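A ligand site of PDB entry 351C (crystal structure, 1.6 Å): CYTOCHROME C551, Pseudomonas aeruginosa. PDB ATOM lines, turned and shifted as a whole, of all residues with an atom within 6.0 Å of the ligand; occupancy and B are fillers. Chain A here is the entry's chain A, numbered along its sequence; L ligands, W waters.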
ATOM      1  N   LEU A   6       4.358  -9.777  16.334  1.00  0.00           N
ATOM      2  CA  LEU A   6       4.985 -10.468  15.209  1.00  0.00           C
ATOM      3  C   LEU A   6       4.455 -11.886  15.056  1.00  0.00           C
ATOM      4  O   LEU A   6       4.243 -12.352  13.936  1.00  0.00           O
ATOM      5  CB  LEU A   6       6.495 -10.539  15.411  1.00  0.00           C
ATOM      6  CG  LEU A   6       7.181  -9.194  15.188  1.00  0.00           C
ATOM      7  CD1 LEU A   6       8.642  -9.234  15.612  1.00  0.00           C
ATOM      8  CD2 LEU A   6       7.036  -8.711  13.737  1.00  0.00           C
ATOM      9  N   PHE A   7       4.334 -12.567  16.183  1.00  0.00           N
ATOM     10  CA  PHE A   7       3.903 -13.971  16.188  1.00  0.00           C
ATOM     11  C   PHE A   7       2.567 -14.159  15.461  1.00  0.00           C
ATOM     12  O   PHE A   7       2.414 -15.080  14.639  1.00  0.00           O
ATOM     13  CB  PHE A   7       3.791 -14.427  17.640  1.00  0.00           C
ATOM     14  CG  PHE A   7       3.081 -15.745  17.875  1.00  0.00           C
ATOM     15  CD1 PHE A   7       1.856 -15.757  18.509  1.00  0.00           C
ATOM     16  CD2 PHE A   7       3.662 -16.928  17.463  1.00  0.00           C
ATOM     17  CE1 PHE A   7       1.194 -16.973  18.762  1.00  0.00           C
ATOM     18  CE2 PHE A   7       3.016 -18.150  17.701  1.00  0.00           C
ATOM     19  CZ  PHE A   7       1.775 -18.173  18.364  1.00  0.00           C
ATOM     20  N   LYS A  10       3.091 -12.287  11.402  1.00  0.00           N
ATOM     21  CA  LYS A  10       3.920 -12.994  10.409  1.00  0.00           C
ATOM     22  C   LYS A  10       3.433 -14.425  10.148  1.00  0.00           C
ATOM     23  O   LYS A  10       4.077 -15.179   9.405  1.00  0.00           O
ATOM     24  CB  LYS A  10       5.354 -13.046  10.897  1.00  0.00           C
ATOM     25  CG  LYS A  10       5.924 -11.650  11.064  1.00  0.00           C
ATOM     26  CD  LYS A  10       6.107 -10.983   9.707  1.00  0.00           C
ATOM     27  CE  LYS A  10       6.688  -9.580   9.868  1.00  0.00           C
ATOM     28  NZ  LYS A  10       7.105  -9.061   8.553  1.00  0.00           N
ATOM     29  N   GLY A  11       2.260 -14.743  10.668  1.00  0.00           N
ATOM     30  CA  GLY A  11       1.638 -16.052  10.361  1.00  0.00           C
ATOM     31  C   GLY A  11       2.163 -17.250  11.155  1.00  0.00           C
ATOM     32  O   GLY A  11       1.793 -18.391  10.830  1.00  0.00           O
ATOM     33  N   CYS A  12       3.075 -17.000  12.098  1.00  0.00           N
ATOM     34  CA  CYS A  12       3.649 -18.105  12.922  1.00  0.00           C
ATOM     35  C   CYS A  12       2.547 -18.885  13.630  1.00  0.00           C
ATOM     36  O   CYS A  12       2.648 -20.102  13.814  1.00  0.00           O
ATOM     37  CB  CYS A  12       4.496 -17.506  14.018  1.00  0.00           C
ATOM     38  SG  CYS A  12       5.689 -16.293  13.427  1.00  0.00           S
ATOM     39  N   VAL A  13       1.526 -18.121  14.031  1.00  0.00           N
ATOM     40  CA  VAL A  13       0.375 -18.643  14.788  1.00  0.00           C
ATOM     41  C   VAL A  13      -0.406 -19.727  14.037  1.00  0.00           C
ATOM     42  O   VAL A  13      -1.085 -20.564  14.635  1.00  0.00           O
ATOM     43  CB  VAL A  13      -0.544 -17.471  15.170  1.00  0.00           C
ATOM     44  CG1 VAL A  13      -1.252 -16.893  13.951  1.00  0.00           C
ATOM     45  CG2 VAL A  13      -1.508 -17.783  16.296  1.00  0.00           C
ATOM     46  N   ALA A  14      -0.213 -19.778  12.726  1.00  0.00           N
ATOM     47  CA  ALA A  14      -0.897 -20.803  11.933  1.00  0.00           C
ATOM     48  C   ALA A  14      -0.295 -22.197  12.112  1.00  0.00           C
ATOM     49  O   ALA A  14      -0.948 -23.182  11.792  1.00  0.00           O
ATOM     50  CB  ALA A  14      -0.854 -20.447  10.459  1.00  0.00           C
ATOM     51  N   CYS A  15       0.968 -22.245  12.515  1.00  0.00           N
ATOM     52  CA  CYS A  15       1.683 -23.541  12.606  1.00  0.00           C
ATOM     53  C   CYS A  15       2.222 -23.843  14.004  1.00  0.00           C
ATOM     54  O   CYS A  15       2.824 -24.901  14.232  1.00  0.00           O
ATOM     55  CB  CYS A  15       2.871 -23.550  11.657  1.00  0.00           C
ATOM     56  SG  CYS A  15       2.389 -23.539   9.917  1.00  0.00           S
ATOM     57  N   HIS A  16       2.182 -22.842  14.870  1.00  0.00           N
ATOM     58  CA  HIS A  16       2.778 -23.025  16.193  1.00  0.00           C
ATOM     59  C   HIS A  16       1.862 -22.544  17.313  1.00  0.00           C
ATOM     60  O   HIS A  16       1.260 -21.470  17.188  1.00  0.00           O
ATOM     61  CB  HIS A  16       4.077 -22.233  16.275  1.00  0.00           C
ATOM     62  CG  HIS A  16       5.244 -22.750  15.446  1.00  0.00           C
ATOM     63  ND1 HIS A  16       6.044 -23.759  15.859  1.00  0.00           N
ATOM     64  CD2 HIS A  16       5.761 -22.241  14.272  1.00  0.00           C
ATOM     65  CE1 HIS A  16       7.047 -23.898  14.952  1.00  0.00           C
ATOM     66  NE2 HIS A  16       6.869 -22.963  13.964  1.00  0.00           N
ATOM     67  N   VAL A  23       1.456 -27.733  13.605  1.00  0.00           N
ATOM     68  CA  VAL A  23       2.241 -28.184  12.446  1.00  0.00           C
ATOM     69  C   VAL A  23       3.737 -28.250  12.746  1.00  0.00           C
ATOM     70  O   VAL A  23       4.376 -29.283  12.510  1.00  0.00           O
ATOM     71  CB  VAL A  23       2.017 -27.261  11.260  1.00  0.00           C
ATOM     72  CG1 VAL A  23       2.829 -27.718  10.051  1.00  0.00           C
ATOM     73  CG2 VAL A  23       0.539 -27.088  10.943  1.00  0.00           C
ATOM     74  N   GLY A  24       4.220 -27.225  13.422  1.00  0.00           N
ATOM     75  CA  GLY A  24       5.595 -27.274  13.928  1.00  0.00           C
ATOM     76  C   GLY A  24       5.584 -27.488  15.449  1.00  0.00           C
ATOM     77  O   GLY A  24       4.516 -27.545  16.074  1.00  0.00           O
ATOM     78  N   PRO A  25       6.753 -27.613  16.035  1.00  0.00           N
ATOM     79  CA  PRO A  25       6.918 -27.849  17.483  1.00  0.00           C
ATOM     80  C   PRO A  25       6.297 -26.762  18.365  1.00  0.00           C
ATOM     81  O   PRO A  25       6.238 -25.599  17.988  1.00  0.00           O
ATOM     82  CB  PRO A  25       8.419 -27.884  17.701  1.00  0.00           C
ATOM     83  CG  PRO A  25       9.018 -27.196  16.497  1.00  0.00           C
ATOM     84  CD  PRO A  25       8.062 -27.500  15.354  1.00  0.00           C
ATOM     85  N   TYR A  27       6.553 -24.035  21.244  1.00  0.00           N
ATOM     86  CA  TYR A  27       7.675 -23.182  21.678  1.00  0.00           C
ATOM     87  C   TYR A  27       8.293 -23.540  23.020  1.00  0.00           C
ATOM     88  O   TYR A  27       9.521 -23.496  23.147  1.00  0.00           O
ATOM     89  CB  TYR A  27       7.375 -21.683  21.596  1.00  0.00           C
ATOM     90  CG  TYR A  27       7.134 -21.121  20.202  1.00  0.00           C
ATOM     91  CD1 TYR A  27       6.239 -20.095  20.008  1.00  0.00           C
ATOM     92  CD2 TYR A  27       7.778 -21.689  19.121  1.00  0.00           C
ATOM     93  CE1 TYR A  27       5.974 -19.630  18.715  1.00  0.00           C
ATOM     94  CE2 TYR A  27       7.517 -21.246  17.821  1.00  0.00           C
ATOM     95  CZ  TYR A  27       6.611 -20.211  17.618  1.00  0.00           C
ATOM     96  OH  TYR A  27       6.330 -19.818  16.399  1.00  0.00           O
ATOM     97  N   VAL A  30      10.819 -26.119  22.204  1.00  0.00           N
ATOM     98  CA  VAL A  30      12.005 -25.557  21.546  1.00  0.00           C
ATOM     99  C   VAL A  30      12.920 -24.884  22.562  1.00  0.00           C
ATOM    100  O   VAL A  30      14.134 -25.115  22.579  1.00  0.00           O
ATOM    101  CB  VAL A  30      11.608 -24.540  20.470  1.00  0.00           C
ATOM    102  CG1 VAL A  30      12.843 -23.918  19.827  1.00  0.00           C
ATOM    103  CG2 VAL A  30      10.737 -25.191  19.403  1.00  0.00           C
ATOM    104  N   LYS A  33      14.743 -27.499  24.592  1.00  0.00           N
ATOM    105  CA  LYS A  33      15.898 -28.088  23.889  1.00  0.00           C
ATOM    106  C   LYS A  33      17.067 -27.115  23.825  1.00  0.00           C
ATOM    107  O   LYS A  33      18.231 -27.488  24.036  1.00  0.00           O
ATOM    108  CB  LYS A  33      15.520 -28.501  22.468  1.00  0.00           C
ATOM    109  CG  LYS A  33      16.714 -29.078  21.708  1.00  0.00           C
ATOM    110  CD  LYS A  33      16.346 -29.683  20.355  1.00  0.00           C
ATOM    111  CE  LYS A  33      15.474 -30.923  20.476  1.00  0.00           C
ATOM    112  NZ  LYS A  33      15.081 -31.417  19.141  1.00  0.00           N
ATOM    113  N   PHE A  34      16.777 -25.890  23.485  1.00  0.00           N
ATOM    114  CA  PHE A  34      17.930 -25.021  23.245  1.00  0.00           C
ATOM    115  C   PHE A  34      18.293 -24.254  24.491  1.00  0.00           C
ATOM    116  O   PHE A  34      19.312 -23.560  24.477  1.00  0.00           O
ATOM    117  CB  PHE A  34      17.679 -24.117  22.051  1.00  0.00           C
ATOM    118  CG  PHE A  34      17.606 -24.940  20.788  1.00  0.00           C
ATOM    119  CD1 PHE A  34      16.398 -25.134  20.151  1.00  0.00           C
ATOM    120  CD2 PHE A  34      18.742 -25.580  20.326  1.00  0.00           C
ATOM    121  CE1 PHE A  34      16.321 -25.963  19.030  1.00  0.00           C
ATOM    122  CE2 PHE A  34      18.684 -26.412  19.200  1.00  0.00           C
ATOM    123  CZ  PHE A  34      17.463 -26.607  18.556  1.00  0.00           C
ATOM    124  N   GLU A  43      21.231 -18.883  15.959  1.00  0.00           N
ATOM    125  CA  GLU A  43      20.960 -20.059  15.131  1.00  0.00           C
ATOM    126  C   GLU A  43      19.471 -20.300  14.858  1.00  0.00           C
ATOM    127  O   GLU A  43      19.071 -20.457  13.702  1.00  0.00           O
ATOM    128  CB  GLU A  43      21.745 -21.261  15.640  1.00  0.00           C
ATOM    129  CG  GLU A  43      23.216 -20.872  15.578  1.00  0.00           C
ATOM    130  CD  GLU A  43      24.187 -22.035  15.766  1.00  0.00           C
ATOM    131  OE1 GLU A  43      25.034 -21.933  16.663  1.00  0.00           O
ATOM    132  OE2 GLU A  43      24.323 -22.821  14.814  1.00  0.00           O
ATOM    133  N   LEU A  44      18.675 -20.036  15.888  1.00  0.00           N
ATOM    134  CA  LEU A  44      17.230 -20.075  15.657  1.00  0.00           C
ATOM    135  C   LEU A  44      16.781 -18.950  14.736  1.00  0.00           C
ATOM    136  O   LEU A  44      15.900 -19.163  13.914  1.00  0.00           O
ATOM    137  CB  LEU A  44      16.448 -19.943  16.955  1.00  0.00           C
ATOM    138  CG  LEU A  44      16.368 -21.219  17.762  1.00  0.00           C
ATOM    139  CD1 LEU A  44      15.449 -21.052  18.958  1.00  0.00           C
ATOM    140  CD2 LEU A  44      15.919 -22.380  16.890  1.00  0.00           C
ATOM    141  N   ARG A  47      17.143 -19.925  11.222  1.00  0.00           N
ATOM    142  CA  ARG A  47      16.187 -20.946  10.790  1.00  0.00           C
ATOM    143  C   ARG A  47      14.780 -20.374  10.658  1.00  0.00           C
ATOM    144  O   ARG A  47      14.040 -20.746   9.739  1.00  0.00           O
ATOM    145  CB  ARG A  47      16.208 -22.163  11.725  1.00  0.00           C
ATOM    146  CG  ARG A  47      17.581 -22.836  11.772  1.00  0.00           C
ATOM    147  CD  ARG A  47      17.623 -24.147  12.548  1.00  0.00           C
ATOM    148  NE  ARG A  47      18.954 -24.315  13.178  1.00  0.00           N
ATOM    149  CZ  ARG A  47      19.277 -25.064  14.243  1.00  0.00           C
ATOM    150  NH1 ARG A  47      20.504 -24.966  14.712  1.00  0.00           N
ATOM    151  NH2 ARG A  47      18.422 -25.861  14.899  1.00  0.00           N
ATOM    152  N   ILE A  48      14.449 -19.429  11.510  1.00  0.00           N
ATOM    153  CA  ILE A  48      13.139 -18.762  11.349  1.00  0.00           C
ATOM    154  C   ILE A  48      13.059 -18.021  10.017  1.00  0.00           C
ATOM    155  O   ILE A  48      12.078 -18.149   9.273  1.00  0.00           O
ATOM    156  CB  ILE A  48      12.895 -17.787  12.498  1.00  0.00           C
ATOM    157  CG1 ILE A  48      12.810 -18.549  13.823  1.00  0.00           C
ATOM    158  CG2 ILE A  48      11.689 -16.875  12.298  1.00  0.00           C
ATOM    159  CD1 ILE A  48      12.770 -17.614  15.012  1.00  0.00           C
ATOM    160  N   SER A  52      13.676 -24.350   7.916  1.00  0.00           N
ATOM    161  CA  SER A  52      14.272 -25.447   8.699  1.00  0.00           C
ATOM    162  C   SER A  52      13.712 -26.796   8.263  1.00  0.00           C
ATOM    163  O   SER A  52      12.535 -26.879   7.925  1.00  0.00           O
ATOM    164  CB  SER A  52      13.948 -25.232  10.177  1.00  0.00           C
ATOM    165  OG  SER A  52      14.658 -26.189  10.960  1.00  0.00           O
ATOM    166  N   GLN A  53      14.498 -27.854   8.391  1.00  0.00           N
ATOM    167  CA  GLN A  53      13.963 -29.215   8.174  1.00  0.00           C
ATOM    168  C   GLN A  53      14.788 -30.256   8.937  1.00  0.00           C
ATOM    169  O   GLN A  53      16.014 -30.160   8.938  1.00  0.00           O
ATOM    170  CB  GLN A  53      13.968 -29.584   6.688  1.00  0.00           C
ATOM    171  CG  GLN A  53      13.174 -30.867   6.430  1.00  0.00           C
ATOM    172  CD  GLN A  53      13.101 -31.195   4.939  1.00  0.00           C
ATOM    173  OE1 GLN A  53      12.678 -32.295   4.581  1.00  0.00           O
ATOM    174  NE2 GLN A  53      13.187 -30.174   4.117  1.00  0.00           N
ATOM    175  N   GLY A  54      14.134 -31.257   9.518  1.00  0.00           N
ATOM    176  CA  GLY A  54      14.928 -32.384  10.042  1.00  0.00           C
ATOM    177  C   GLY A  54      15.170 -32.326  11.545  1.00  0.00           C
ATOM    178  O   GLY A  54      15.513 -33.346  12.157  1.00  0.00           O
ATOM    179  N   VAL A  55      15.029 -31.149  12.140  1.00  0.00           N
ATOM    180  CA  VAL A  55      15.322 -31.080  13.593  1.00  0.00           C
ATOM    181  C   VAL A  55      14.207 -31.674  14.460  1.00  0.00           C
ATOM    182  O   VAL A  55      14.480 -32.276  15.500  1.00  0.00           O
ATOM    183  CB  VAL A  55      15.647 -29.645  13.989  1.00  0.00           C
ATOM    184  CG1 VAL A  55      16.054 -29.505  15.456  1.00  0.00           C
ATOM    185  CG2 VAL A  55      16.691 -29.056  13.060  1.00  0.00           C
ATOM    186  N   TRP A  56      12.966 -31.447  14.036  1.00  0.00           N
ATOM    187  CA  TRP A  56      11.813 -31.884  14.840  1.00  0.00           C
ATOM    188  C   TRP A  56      10.919 -32.893  14.120  1.00  0.00           C
ATOM    189  O   TRP A  56       9.776 -33.128  14.528  1.00  0.00           O
ATOM    190  CB  TRP A  56      10.948 -30.674  15.197  1.00  0.00           C
ATOM    191  CG  TRP A  56      11.667 -29.678  16.061  1.00  0.00           C
ATOM    192  CD1 TRP A  56      12.434 -28.593  15.673  1.00  0.00           C
ATOM    193  CD2 TRP A  56      11.756 -29.708  17.459  1.00  0.00           C
ATOM    194  NE1 TRP A  56      12.956 -28.006  16.789  1.00  0.00           N
ATOM    195  CE2 TRP A  56      12.581 -28.629  17.834  1.00  0.00           C
ATOM    196  CE3 TRP A  56      11.201 -30.559  18.405  1.00  0.00           C
ATOM    197  CZ2 TRP A  56      12.894 -28.347  19.152  1.00  0.00           C
ATOM    198  CZ3 TRP A  56      11.516 -30.292  19.747  1.00  0.00           C
ATOM    199  CH2 TRP A  56      12.331 -29.204  20.113  1.00  0.00           C
ATOM    200  N   GLY A  57      11.415 -33.330  12.974  1.00  0.00           N
ATOM    201  CA  GLY A  57      10.597 -34.180  12.101  1.00  0.00           C
ATOM    202  C   GLY A  57      10.941 -33.916  10.637  1.00  0.00           C
ATOM    203  O   GLY A  57      11.893 -33.179  10.379  1.00  0.00           O
ATOM    204  N   PRO A  58      10.290 -34.631   9.727  1.00  0.00           N
ATOM    205  CA  PRO A  58      10.678 -34.674   8.311  1.00  0.00           C
ATOM    206  C   PRO A  58      10.102 -33.502   7.506  1.00  0.00           C
ATOM    207  O   PRO A  58      10.433 -33.363   6.327  1.00  0.00           O
ATOM    208  CB  PRO A  58      10.053 -35.963   7.787  1.00  0.00           C
ATOM    209  CG  PRO A  58       8.837 -36.179   8.652  1.00  0.00           C
ATOM    210  CD  PRO A  58       9.274 -35.672  10.023  1.00  0.00           C
ATOM    211  N   ILE A  59       9.168 -32.757   8.087  1.00  0.00           N
ATOM    212  CA  ILE A  59       8.499 -31.702   7.303  1.00  0.00           C
ATOM    213  C   ILE A  59       9.095 -30.333   7.585  1.00  0.00           C
ATOM    214  O   ILE A  59       9.570 -30.063   8.694  1.00  0.00           O
ATOM    215  CB  ILE A  59       6.990 -31.689   7.498  1.00  0.00           C
ATOM    216  CG1 ILE A  59       6.573 -31.174   8.870  1.00  0.00           C
ATOM    217  CG2 ILE A  59       6.344 -33.012   7.116  1.00  0.00           C
ATOM    218  CD1 ILE A  59       5.112 -30.753   8.850  1.00  0.00           C
ATOM    219  N   PRO A  60       9.238 -29.553   6.537  1.00  0.00           N
ATOM    220  CA  PRO A  60       9.995 -28.293   6.598  1.00  0.00           C
ATOM    221  C   PRO A  60       9.166 -27.156   7.183  1.00  0.00           C
ATOM    222  O   PRO A  60       7.964 -27.033   6.907  1.00  0.00           O
ATOM    223  CB  PRO A  60      10.301 -27.969   5.144  1.00  0.00           C
ATOM    224  CG  PRO A  60       9.144 -28.566   4.380  1.00  0.00           C
ATOM    225  CD  PRO A  60       8.784 -29.821   5.154  1.00  0.00           C
ATOM    226  N   MET A  61       9.883 -26.253   7.799  1.00  0.00           N
ATOM    227  CA  MET A  61       9.342 -24.891   7.949  1.00  0.00           C
ATOM    228  C   MET A  61       9.821 -24.097   6.729  1.00  0.00           C
ATOM    229  O   MET A  61      11.031 -23.983   6.538  1.00  0.00           O
ATOM    230  CB  MET A  61       9.936 -24.194   9.169  1.00  0.00           C
ATOM    231  CG  MET A  61       9.403 -22.757   9.247  1.00  0.00           C
ATOM    232  SD  MET A  61       9.689 -21.928  10.825  1.00  0.00           S
ATOM    233  CE  MET A  61      11.395 -22.314  11.253  1.00  0.00           C
ATOM    234  N   PRO A  62       8.885 -23.650   5.897  1.00  0.00           N
ATOM    235  CA  PRO A  62       9.192 -22.805   4.742  1.00  0.00           C
ATOM    236  C   PRO A  62       9.826 -21.490   5.204  1.00  0.00           C
ATOM    237  O   PRO A  62       9.591 -21.070   6.346  1.00  0.00           O
ATOM    238  CB  PRO A  62       7.839 -22.488   4.111  1.00  0.00           C
ATOM    239  CG  PRO A  62       6.873 -23.491   4.715  1.00  0.00           C
ATOM    240  CD  PRO A  62       7.434 -23.760   6.088  1.00  0.00           C
ATOM    241  N   ASN A  64      10.356 -17.658   5.946  1.00  0.00           N
ATOM    242  CA  ASN A  64       9.382 -16.673   6.426  1.00  0.00           C
ATOM    243  C   ASN A  64       9.654 -15.292   5.856  1.00  0.00           C
ATOM    244  O   ASN A  64      10.782 -14.999   5.463  1.00  0.00           O
ATOM    245  CB  ASN A  64       9.398 -16.617   7.958  1.00  0.00           C
ATOM    246  CG  ASN A  64       8.671 -17.841   8.521  1.00  0.00           C
ATOM    247  OD1 ASN A  64       7.461 -17.983   8.343  1.00  0.00           O
ATOM    248  ND2 ASN A  64       9.412 -18.731   9.131  1.00  0.00           N
ATOM    249  N   VAL A  66      10.142 -12.446   7.089  1.00  0.00           N
ATOM    250  CA  VAL A  66      10.608 -11.621   8.205  1.00  0.00           C
ATOM    251  C   VAL A  66      11.972 -11.010   7.887  1.00  0.00           C
ATOM    252  O   VAL A  66      12.744 -11.588   7.131  1.00  0.00           O
ATOM    253  CB  VAL A  66      10.697 -12.434   9.507  1.00  0.00           C
ATOM    254  CG1 VAL A  66       9.344 -12.784  10.089  1.00  0.00           C
ATOM    255  CG2 VAL A  66      11.643 -13.635   9.400  1.00  0.00           C
ATOM    256  N   LEU A  74      12.023 -12.614  17.467  1.00  0.00           N
ATOM    257  CA  LEU A  74      11.198 -13.804  17.605  1.00  0.00           C
ATOM    258  C   LEU A  74      11.986 -14.954  18.242  1.00  0.00           C
ATOM    259  O   LEU A  74      11.459 -15.638  19.124  1.00  0.00           O
ATOM    260  CB  LEU A  74      10.663 -14.223  16.236  1.00  0.00           C
ATOM    261  CG  LEU A  74       9.441 -13.430  15.797  1.00  0.00           C
ATOM    262  CD1 LEU A  74       9.197 -13.550  14.296  1.00  0.00           C
ATOM    263  CD2 LEU A  74       8.195 -13.787  16.582  1.00  0.00           C
ATOM    264  N   ALA A  75      13.231 -15.096  17.836  1.00  0.00           N
ATOM    265  CA  ALA A  75      14.063 -16.189  18.395  1.00  0.00           C
ATOM    266  C   ALA A  75      14.255 -16.019  19.902  1.00  0.00           C
ATOM    267  O   ALA A  75      14.076 -16.967  20.674  1.00  0.00           O
ATOM    268  CB  ALA A  75      15.424 -16.203  17.734  1.00  0.00           C
ATOM    269  N   VAL A  78      10.970 -16.882  21.667  1.00  0.00           N
ATOM    270  CA  VAL A  78      10.767 -18.336  21.727  1.00  0.00           C
ATOM    271  C   VAL A  78      11.625 -18.988  22.818  1.00  0.00           C
ATOM    272  O   VAL A  78      11.124 -19.765  23.635  1.00  0.00           O
ATOM    273  CB  VAL A  78      11.069 -18.982  20.386  1.00  0.00           C
ATOM    274  CG1 VAL A  78      11.184 -20.507  20.468  1.00  0.00           C
ATOM    275  CG2 VAL A  78      10.072 -18.566  19.313  1.00  0.00           C
HETATM  276  C1  LIG L   1      10.325 -25.054  13.471  1.00  0.00           C
HETATM  277  C2  LIG L   1       9.722 -20.424  14.642  1.00  0.00           C
HETATM  278  C3  LIG L   1       6.288 -20.022  11.274  1.00  0.00           C
HETATM  279  C4  LIG L   1       6.488 -24.777  10.544  1.00  0.00           C
HETATM  280  C5  LIG L   1      10.476 -23.829  14.093  1.00  0.00           C
HETATM  281  C6  LIG L   1      11.397 -23.521  15.065  1.00  0.00           C
HETATM  282  C7  LIG L   1      11.173 -22.209  15.445  1.00  0.00           C
HETATM  283  C8  LIG L   1      10.178 -21.718  14.634  1.00  0.00           C
HETATM  284  C9  LIG L   1      11.886 -21.419  16.523  1.00  0.00           C
HETATM  285  C10 LIG L   1      12.463 -24.442  15.611  1.00  0.00           C
HETATM  286  C11 LIG L   1      13.638 -24.409  14.657  1.00  0.00           C
HETATM  287  C12 LIG L   1      14.745 -25.326  15.157  1.00  0.00           C
HETATM  288  O1  LIG L   1      14.580 -25.924  16.217  1.00  0.00           O
HETATM  289  O2  LIG L   1      15.943 -24.926  14.901  1.00  0.00           O
HETATM  290  C13 LIG L   1       8.709 -19.902  13.862  1.00  0.00           C
HETATM  291  C14 LIG L   1       8.336 -18.558  13.824  1.00  0.00           C
HETATM  292  C15 LIG L   1       7.416 -18.415  12.781  1.00  0.00           C
HETATM  293  C16 LIG L   1       7.180 -19.701  12.284  1.00  0.00           C
HETATM  294  C17 LIG L   1       8.896 -17.457  14.683  1.00  0.00           C
HETATM  295  C18 LIG L   1       6.791 -17.135  12.259  1.00  0.00           C
HETATM  296  C19 LIG L   1       7.780 -16.160  11.642  1.00  0.00           C
HETATM  297  C20 LIG L   1       6.063 -21.283  10.758  1.00  0.00           C
HETATM  298  C21 LIG L   1       5.086 -21.604   9.827  1.00  0.00           C
HETATM  299  C22 LIG L   1       5.041 -22.980   9.748  1.00  0.00           C
HETATM  300  C23 LIG L   1       6.112 -23.460  10.480  1.00  0.00           C
HETATM  301  C24 LIG L   1       4.116 -20.666   9.152  1.00  0.00           C
HETATM  302  C25 LIG L   1       3.984 -23.801   9.062  1.00  0.00           C
HETATM  303  C26 LIG L   1       3.954 -23.702   7.556  1.00  0.00           C
HETATM  304  C27 LIG L   1       7.563 -25.263  11.255  1.00  0.00           C
HETATM  305  C28 LIG L   1       7.990 -26.586  11.240  1.00  0.00           C
HETATM  306  C29 LIG L   1       9.149 -26.644  12.008  1.00  0.00           C
HETATM  307  C30 LIG L   1       9.342 -25.371  12.553  1.00  0.00           C
HETATM  308  C31 LIG L   1       7.326 -27.727  10.495  1.00  0.00           C
HETATM  309  C32 LIG L   1      10.032 -27.842  12.251  1.00  0.00           C
HETATM  310  C33 LIG L   1      11.261 -27.833  11.360  1.00  0.00           C
HETATM  311  C34 LIG L   1      12.170 -29.014  11.688  1.00  0.00           C
HETATM  312  O3  LIG L   1      13.387 -28.887  11.514  1.00  0.00           O
HETATM  313  O4  LIG L   1      11.683 -30.220  11.915  1.00  0.00           O
HETATM  314  N1  LIG L   1       9.741 -22.725  13.844  1.00  0.00           N
HETATM  315  N2  LIG L   1       7.992 -20.593  12.925  1.00  0.00           N
HETATM  316  N3  LIG L   1       6.677 -22.430  11.139  1.00  0.00           N
HETATM  317  N4  LIG L   1       8.385 -24.522  12.073  1.00  0.00           N
HETATM  318 FE1  LIG L   1       8.165 -22.596  12.499  1.00  0.00          FE
HETATM  319  O   HOH W   1       9.422 -31.154  11.087  1.00  0.00           O
HETATM  320  O   HOH W   2       7.161 -20.770   7.210  1.00  0.00           O
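SG of Cys 12 is covalently linked to C18 of the ligand, 1.8 Å away.
The side-chain sulfur (SG) of Cys 15 is bonded to a carbon (C25) of the ligand (1.8 Å).
A ring nitrogen (NE2) of His 16 is bound to an iron atom (FE1) of the ligand (2.0 Å).
The side-chain sulfur (SD) of Met 61 is bound to an iron atom (FE1) of the ligand, at 2.4 Å.
The guanidinium group (NH2) of Arg 47 is in salt-bridge range of an oxygen (O2) of the ligand, at 2.6 Å.
N of Trp 56 sits at hydrogen-bond distance from O4 of the ligand (2.8 Å).
NE1 of Trp 56 sits at hydrogen-bond distance from O1 of the ligand (2.7 Å).
An oxygen (O3) of the ligand sits at hydrogen-bond distance from the backbone NH of Val 55 (2.9 Å).
O3 of the ligand lies within hydrogen-bond range of OG of Ser 52 (3.0 Å).
N of Gly 54 is in hydrogen-bond range of O3 of the ligand (3.2 Å).
An oxygen (O3) of the ligand sits close to the backbone NH of Gln 53.
The backbone NH of Gly 57 sits at hydrogen-bond distance from an oxygen (O4) of the ligand (3.3 Å).
O of Phe 7 lies within hydrogen-bond range of N of Cys 12 (3.3 Å).
N of Gly 24 lies within hydrogen-bond range of O of Cys 15.
The backbone carbonyl oxygen (O) of Cys 15 is in hydrogen-bond range of the backbone NH (N) of Val 23 (3.2 Å).
A ring nitrogen (ND1) of His 16 is in hydrogen-bond range of the backbone carbonyl oxygen (O) of Pro 25, at 2.8 Å.
The backbone NH of Met 61 lies within hydrogen-bond range of the backbone carbonyl oxygen of Ser 52 (2.7 Å).
SD of Met 61 lies close to ND2 of Asn 64, 3.6 Å away.
OE1 of Gln 53 sits close to O of Pro 58.
ND2 of Asn 64 sits at hydrogen-bond distance from O of Ile 48 (2.7 Å).
Residues that only touch the ligand: Gly 11, Val 23, Gly 24, Pro 25, Tyr 27, Phe 34, Leu 44, Ile 48, Ile 59, Pro 60, Pro 62, Asn 64 and Leu 74.
Hydrophobic or aromatic side chains within 4 Å of the ligand: His 16, Pro 25, Tyr 27, Phe 34, Leu 44, Ile 48, Val 55, Trp 56, Ile 59, Met 61, Pro 62 and Leu 74.
24 residues have an atom within 4 Å of the ligand: Gly 11, Cys 12, Cys 15, His 16, Val 23, Gly 24, Pro 25, Tyr 27, Phe 34, Leu 44, Arg 47, Ile 48, Ser 52, Gln 53, Gly 54, Val 55, Trp 56, Gly 57, Ile 59, Pro 60, Met 61, Pro 62, Asn 64 and Leu 74.
Along chain A the residues within 4 Å of the ligand span positions 11 to 74.
Water W1 lies within hydrogen-bond range of O4 of the ligand (2.6 Å), O of Ile 59 (2.6 Å) and O of Gly 57 (3.3 Å).
Water W2 lies within hydrogen-bond range of the backbone carbonyl oxygen of Pro 62 (2.6 Å) and the side-chain amide oxygen of Asn 64 (3.0 Å).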
